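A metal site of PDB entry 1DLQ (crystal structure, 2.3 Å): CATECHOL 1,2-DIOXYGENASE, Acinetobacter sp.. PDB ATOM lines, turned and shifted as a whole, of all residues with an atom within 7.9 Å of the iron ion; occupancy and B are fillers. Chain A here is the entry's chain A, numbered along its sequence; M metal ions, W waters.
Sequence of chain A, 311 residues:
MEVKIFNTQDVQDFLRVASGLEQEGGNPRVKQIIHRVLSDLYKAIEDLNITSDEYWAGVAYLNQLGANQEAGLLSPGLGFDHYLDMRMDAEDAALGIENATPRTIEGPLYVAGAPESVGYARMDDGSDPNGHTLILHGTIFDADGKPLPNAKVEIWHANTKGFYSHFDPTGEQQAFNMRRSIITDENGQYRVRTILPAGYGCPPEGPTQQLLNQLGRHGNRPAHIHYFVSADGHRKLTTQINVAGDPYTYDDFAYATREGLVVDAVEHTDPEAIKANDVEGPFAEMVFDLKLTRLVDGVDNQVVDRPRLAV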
ATOM      1  N   ILE A 105      -9.538 -21.419  19.061  1.00  0.00           N
ATOM      2  CA  ILE A 105      -9.296 -20.090  18.496  1.00  0.00           C
ATOM      3  C   ILE A 105      -9.777 -19.820  17.074  1.00  0.00           C
ATOM      4  O   ILE A 105      -9.864 -20.711  16.236  1.00  0.00           O
ATOM      5  CB  ILE A 105      -7.800 -19.686  18.609  1.00  0.00           C
ATOM      6  CG1 ILE A 105      -6.960 -20.372  17.538  1.00  0.00           C
ATOM      7  CG2 ILE A 105      -7.262 -20.086  19.987  1.00  0.00           C
ATOM      8  CD1 ILE A 105      -5.540 -19.842  17.492  1.00  0.00           C
ATOM      9  N   GLU A 106     -10.114 -18.552  16.844  1.00  0.00           N
ATOM     10  CA  GLU A 106     -10.585 -18.098  15.551  1.00  0.00           C
ATOM     11  C   GLU A 106      -9.451 -17.835  14.551  1.00  0.00           C
ATOM     12  O   GLU A 106      -9.615 -18.041  13.346  1.00  0.00           O
ATOM     13  CB  GLU A 106     -11.392 -16.804  15.750  1.00  0.00           C
ATOM     14  CG  GLU A 106     -11.699 -16.033  14.478  1.00  0.00           C
ATOM     15  CD  GLU A 106     -12.416 -14.725  14.767  1.00  0.00           C
ATOM     16  OE1 GLU A 106     -12.887 -14.546  15.918  1.00  0.00           O
ATOM     17  OE2 GLU A 106     -12.520 -13.890  13.844  1.00  0.00           O
ATOM     18  N   GLY A 107      -8.298 -17.403  15.046  1.00  0.00           N
ATOM     19  CA  GLY A 107      -7.212 -17.098  14.123  1.00  0.00           C
ATOM     20  C   GLY A 107      -7.444 -15.704  13.560  1.00  0.00           C
ATOM     21  O   GLY A 107      -8.553 -15.162  13.672  1.00  0.00           O
ATOM     22  N   PRO A 108      -6.425 -15.063  12.979  1.00  0.00           N
ATOM     23  CA  PRO A 108      -6.594 -13.716  12.432  1.00  0.00           C
ATOM     24  C   PRO A 108      -6.989 -13.638  10.947  1.00  0.00           C
ATOM     25  O   PRO A 108      -6.932 -12.561  10.360  1.00  0.00           O
ATOM     26  CB  PRO A 108      -5.218 -13.129  12.660  1.00  0.00           C
ATOM     27  CG  PRO A 108      -4.364 -14.281  12.180  1.00  0.00           C
ATOM     28  CD  PRO A 108      -5.019 -15.485  12.859  1.00  0.00           C
ATOM     29  N   LEU A 109      -7.413 -14.754  10.371  1.00  0.00           N
ATOM     30  CA  LEU A 109      -7.720 -14.780   8.940  1.00  0.00           C
ATOM     31  C   LEU A 109      -9.166 -14.830   8.493  1.00  0.00           C
ATOM     32  O   LEU A 109      -9.451 -15.265   7.371  1.00  0.00           O
ATOM     33  CB  LEU A 109      -6.928 -15.926   8.291  1.00  0.00           C
ATOM     34  CG  LEU A 109      -5.422 -15.830   8.574  1.00  0.00           C
ATOM     35  CD1 LEU A 109      -4.688 -17.035   8.026  1.00  0.00           C
ATOM     36  CD2 LEU A 109      -4.884 -14.541   7.964  1.00  0.00           C
ATOM     37  N   TYR A 110     -10.091 -14.402   9.343  1.00  0.00           N
ATOM     38  CA  TYR A 110     -11.511 -14.406   8.973  1.00  0.00           C
ATOM     39  C   TYR A 110     -11.833 -13.197   8.080  1.00  0.00           C
ATOM     40  O   TYR A 110     -11.321 -12.111   8.305  1.00  0.00           O
ATOM     41  CB  TYR A 110     -12.386 -14.335  10.218  1.00  0.00           C
ATOM     42  CG  TYR A 110     -13.867 -14.156   9.897  1.00  0.00           C
ATOM     43  CD1 TYR A 110     -14.617 -15.183   9.322  1.00  0.00           C
ATOM     44  CD2 TYR A 110     -14.501 -12.944  10.156  1.00  0.00           C
ATOM     45  CE1 TYR A 110     -15.953 -15.003   9.009  1.00  0.00           C
ATOM     46  CE2 TYR A 110     -15.846 -12.759   9.841  1.00  0.00           C
ATOM     47  CZ  TYR A 110     -16.563 -13.790   9.274  1.00  0.00           C
ATOM     48  OH  TYR A 110     -17.887 -13.600   8.977  1.00  0.00           O
ATOM     49  N   TRP A 156     -13.935 -21.315   6.434  1.00  0.00           N
ATOM     50  CA  TRP A 156     -12.827 -20.738   5.693  1.00  0.00           C
ATOM     51  C   TRP A 156     -11.586 -21.564   5.973  1.00  0.00           C
ATOM     52  O   TRP A 156     -11.351 -21.994   7.106  1.00  0.00           O
ATOM     53  CB  TRP A 156     -12.641 -19.238   6.048  1.00  0.00           C
ATOM     54  CG  TRP A 156     -12.131 -18.866   7.437  1.00  0.00           C
ATOM     55  CD1 TRP A 156     -10.865 -18.455   7.777  1.00  0.00           C
ATOM     56  CD2 TRP A 156     -12.907 -18.776   8.641  1.00  0.00           C
ATOM     57  NE1 TRP A 156     -10.805 -18.110   9.110  1.00  0.00           N
ATOM     58  CE2 TRP A 156     -12.045 -18.294   9.660  1.00  0.00           C
ATOM     59  CE3 TRP A 156     -14.250 -19.047   8.972  1.00  0.00           C
ATOM     60  CZ2 TRP A 156     -12.477 -18.081  10.975  1.00  0.00           C
ATOM     61  CZ3 TRP A 156     -14.679 -18.837  10.273  1.00  0.00           C
ATOM     62  CH2 TRP A 156     -13.797 -18.360  11.260  1.00  0.00           C
ATOM     63  N   HIS A 157     -10.826 -21.838   4.918  1.00  0.00           N
ATOM     64  CA  HIS A 157      -9.610 -22.629   5.046  1.00  0.00           C
ATOM     65  C   HIS A 157      -8.624 -22.244   3.946  1.00  0.00           C
ATOM     66  O   HIS A 157      -8.956 -21.508   3.014  1.00  0.00           O
ATOM     67  CB  HIS A 157      -9.935 -24.128   4.998  1.00  0.00           C
ATOM     68  CG  HIS A 157     -10.429 -24.599   3.668  1.00  0.00           C
ATOM     69  ND1 HIS A 157      -9.589 -24.865   2.607  1.00  0.00           N
ATOM     70  CD2 HIS A 157     -11.683 -24.839   3.210  1.00  0.00           C
ATOM     71  CE1 HIS A 157     -10.294 -25.248   1.560  1.00  0.00           C
ATOM     72  NE2 HIS A 157     -11.573 -25.232   1.902  1.00  0.00           N
ATOM     73  N   ALA A 158      -7.397 -22.750   4.060  1.00  0.00           N
ATOM     74  CA  ALA A 158      -6.362 -22.448   3.097  1.00  0.00           C
ATOM     75  C   ALA A 158      -6.313 -23.472   1.975  1.00  0.00           C
ATOM     76  O   ALA A 158      -7.035 -24.479   2.013  1.00  0.00           O
ATOM     77  CB  ALA A 158      -5.021 -22.385   3.813  1.00  0.00           C
ATOM     78  N   GLY A 162      -1.107 -23.586   1.629  1.00  0.00           N
ATOM     79  CA  GLY A 162      -1.294 -22.985   2.932  1.00  0.00           C
ATOM     80  C   GLY A 162      -1.708 -21.530   2.951  1.00  0.00           C
ATOM     81  O   GLY A 162      -1.520 -20.838   3.959  1.00  0.00           O
ATOM     82  N   TYR A 164      -4.680 -18.451   2.435  1.00  0.00           N
ATOM     83  CA  TYR A 164      -6.098 -18.161   2.460  1.00  0.00           C
ATOM     84  C   TYR A 164      -6.309 -17.018   1.478  1.00  0.00           C
ATOM     85  O   TYR A 164      -5.397 -16.225   1.242  1.00  0.00           O
ATOM     86  CB  TYR A 164      -6.579 -17.680   3.832  1.00  0.00           C
ATOM     87  CG  TYR A 164      -6.518 -18.687   4.962  1.00  0.00           C
ATOM     88  CD1 TYR A 164      -5.297 -19.172   5.424  1.00  0.00           C
ATOM     89  CD2 TYR A 164      -7.682 -19.125   5.584  1.00  0.00           C
ATOM     90  CE1 TYR A 164      -5.231 -20.051   6.486  1.00  0.00           C
ATOM     91  CE2 TYR A 164      -7.637 -20.015   6.651  1.00  0.00           C
ATOM     92  CZ  TYR A 164      -6.412 -20.479   7.102  1.00  0.00           C
ATOM     93  OH  TYR A 164      -6.347 -21.358   8.165  1.00  0.00           O
ATOM     94  N   ALA A 198      -3.838 -27.404   3.491  1.00  0.00           N
ATOM     95  CA  ALA A 198      -2.559 -27.883   3.971  1.00  0.00           C
ATOM     96  C   ALA A 198      -2.263 -27.006   5.182  1.00  0.00           C
ATOM     97  O   ALA A 198      -2.868 -25.944   5.336  1.00  0.00           O
ATOM     98  CB  ALA A 198      -1.489 -27.675   2.916  1.00  0.00           C
ATOM     99  N   TYR A 200       0.330 -24.651   7.487  1.00  0.00           N
ATOM    100  CA  TYR A 200       1.122 -23.517   7.035  1.00  0.00           C
ATOM    101  C   TYR A 200       1.883 -22.953   8.215  1.00  0.00           C
ATOM    102  O   TYR A 200       1.539 -23.224   9.361  1.00  0.00           O
ATOM    103  CB  TYR A 200       0.208 -22.446   6.413  1.00  0.00           C
ATOM    104  CG  TYR A 200      -0.906 -21.996   7.321  1.00  0.00           C
ATOM    105  CD1 TYR A 200      -0.688 -21.031   8.306  1.00  0.00           C
ATOM    106  CD2 TYR A 200      -2.175 -22.562   7.215  1.00  0.00           C
ATOM    107  CE1 TYR A 200      -1.711 -20.641   9.157  1.00  0.00           C
ATOM    108  CE2 TYR A 200      -3.208 -22.175   8.057  1.00  0.00           C
ATOM    109  CZ  TYR A 200      -2.973 -21.212   9.024  1.00  0.00           C
ATOM    110  OH  TYR A 200      -3.993 -20.833   9.885  1.00  0.00           O
ATOM    111  N   ARG A 221       1.272 -24.757  11.776  1.00  0.00           N
ATOM    112  CA  ARG A 221      -0.057 -25.167  12.209  1.00  0.00           C
ATOM    113  C   ARG A 221      -0.445 -26.377  11.387  1.00  0.00           C
ATOM    114  O   ARG A 221      -0.124 -26.462  10.200  1.00  0.00           O
ATOM    115  CB  ARG A 221      -1.094 -24.058  11.987  1.00  0.00           C
ATOM    116  CG  ARG A 221      -0.842 -22.757  12.725  1.00  0.00           C
ATOM    117  CD  ARG A 221      -2.156 -22.022  12.895  1.00  0.00           C
ATOM    118  NE  ARG A 221      -3.026 -22.784  13.790  1.00  0.00           N
ATOM    119  CZ  ARG A 221      -4.316 -22.567  13.989  1.00  0.00           C
ATOM    120  NH1 ARG A 221      -4.972 -21.586  13.344  1.00  0.00           N
ATOM    121  NH2 ARG A 221      -4.973 -23.350  14.831  1.00  0.00           N
ATOM    122  N   PRO A 222      -1.139 -27.349  11.991  1.00  0.00           N
ATOM    123  CA  PRO A 222      -1.575 -28.540  11.273  1.00  0.00           C
ATOM    124  C   PRO A 222      -2.729 -28.146  10.335  1.00  0.00           C
ATOM    125  O   PRO A 222      -3.336 -27.088  10.526  1.00  0.00           O
ATOM    126  CB  PRO A 222      -2.052 -29.448  12.406  1.00  0.00           C
ATOM    127  CG  PRO A 222      -2.672 -28.439  13.346  1.00  0.00           C
ATOM    128  CD  PRO A 222      -1.545 -27.433  13.412  1.00  0.00           C
ATOM    129  N   ALA A 223      -3.008 -28.964   9.331  1.00  0.00           N
ATOM    130  CA  ALA A 223      -4.092 -28.657   8.388  1.00  0.00           C
ATOM    131  C   ALA A 223      -5.413 -28.619   9.151  1.00  0.00           C
ATOM    132  O   ALA A 223      -5.719 -29.518   9.937  1.00  0.00           O
ATOM    133  CB  ALA A 223      -4.142 -29.710   7.287  1.00  0.00           C
ATOM    134  N   HIS A 224      -6.198 -27.570   8.907  1.00  0.00           N
ATOM    135  CA  HIS A 224      -7.464 -27.403   9.599  1.00  0.00           C
ATOM    136  C   HIS A 224      -8.456 -26.542   8.822  1.00  0.00           C
ATOM    137  O   HIS A 224      -8.100 -25.824   7.883  1.00  0.00           O
ATOM    138  CB  HIS A 224      -7.237 -26.745  10.938  1.00  0.00           C
ATOM    139  CG  HIS A 224      -6.599 -25.404  10.819  1.00  0.00           C
ATOM    140  ND1 HIS A 224      -5.255 -25.249  10.525  1.00  0.00           N
ATOM    141  CD2 HIS A 224      -7.117 -24.160  10.833  1.00  0.00           C
ATOM    142  CE1 HIS A 224      -4.983 -23.961  10.380  1.00  0.00           C
ATOM    143  NE2 HIS A 224      -6.103 -23.283  10.559  1.00  0.00           N
ATOM    144  N   ILE A 225      -9.705 -26.599   9.266  1.00  0.00           N
ATOM    145  CA  ILE A 225     -10.783 -25.852   8.646  1.00  0.00           C
ATOM    146  C   ILE A 225     -11.488 -25.041   9.731  1.00  0.00           C
ATOM    147  O   ILE A 225     -11.858 -25.586  10.775  1.00  0.00           O
ATOM    148  CB  ILE A 225     -11.771 -26.818   7.949  1.00  0.00           C
ATOM    149  CG1 ILE A 225     -10.987 -27.691   6.953  1.00  0.00           C
ATOM    150  CG2 ILE A 225     -12.876 -26.041   7.244  1.00  0.00           C
ATOM    151  CD1 ILE A 225     -11.787 -28.815   6.318  1.00  0.00           C
ATOM    152  N   HIS A 226     -11.633 -23.745   9.492  1.00  0.00           N
ATOM    153  CA  HIS A 226     -12.276 -22.829  10.438  1.00  0.00           C
ATOM    154  C   HIS A 226     -13.812 -22.805  10.355  1.00  0.00           C
ATOM    155  O   HIS A 226     -14.382 -22.840   9.257  1.00  0.00           O
ATOM    156  CB  HIS A 226     -11.752 -21.412  10.213  1.00  0.00           C
ATOM    157  CG  HIS A 226     -10.309 -21.232  10.547  1.00  0.00           C
ATOM    158  ND1 HIS A 226      -9.862 -20.968  11.818  1.00  0.00           N
ATOM    159  CD2 HIS A 226      -9.204 -21.276   9.760  1.00  0.00           C
ATOM    160  CE1 HIS A 226      -8.553 -20.852  11.811  1.00  0.00           C
ATOM    161  NE2 HIS A 226      -8.118 -21.038  10.572  1.00  0.00           N
ATOM    162  N   GLN A 240     -12.932 -25.208  15.039  1.00  0.00           N
ATOM    163  CA  GLN A 240     -12.267 -25.606  13.817  1.00  0.00           C
ATOM    164  C   GLN A 240     -12.072 -27.118  13.908  1.00  0.00           C
ATOM    165  O   GLN A 240     -12.322 -27.722  14.960  1.00  0.00           O
ATOM    166  CB  GLN A 240     -10.906 -24.925  13.715  1.00  0.00           C
ATOM    167  CG  GLN A 240      -9.821 -25.689  14.428  1.00  0.00           C
ATOM    168  CD  GLN A 240      -8.464 -24.986  14.380  1.00  0.00           C
ATOM    169  OE1 GLN A 240      -7.440 -25.594  14.726  1.00  0.00           O
ATOM    170  NE2 GLN A 240      -8.447 -23.716  13.976  1.00  0.00           N
HETATM  171 FE    FE M   1      -6.161 -21.068  10.006  1.00  0.00          FE
HETATM  172  O   HOH W   1      -5.596 -19.052  10.914  1.00  0.00           O
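The iron ion is bound by the side-chain hydroxyl of Tyr 164 (1.9 Å), a ring nitrogen (NE2) of His 226 (2.0 Å), the side-chain hydroxyl of Tyr 200 (2.2 Å), water W1 (2.3 Å) and a ring nitrogen (NE2) of His 224 (2.3 Å).
Residues that only touch the iron ion: Arg 221 (3.6 Å). The nearest printed residue that does not touch the iron ion is Leu 109 (4.7 Å).
The backbone NH (N) of His 226 is in hydrogen-bond range of the backbone carbonyl oxygen (O) of Trp 156, 3.0 Å away. A ring nitrogen (NE2) of His 224 lies close to the guanidinium group of Arg 221 (3.5 Å). A ring nitrogen (ND1) of His 226 lies within hydrogen-bond range of the backbone carbonyl oxygen (O) of Glu 106, at 3.3 Å. The guanidinium group of Arg 221 sits at hydrogen-bond distance from the side-chain amide oxygen of Gln 240 (3.3 Å). The backbone carbonyl oxygen (O) of Tyr 200 is in hydrogen-bond range of the backbone NH (N) of Arg 221, at 2.9 Å. ND1 of His 224 lies within hydrogen-bond range of O of Pro 222 (2.7 Å).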
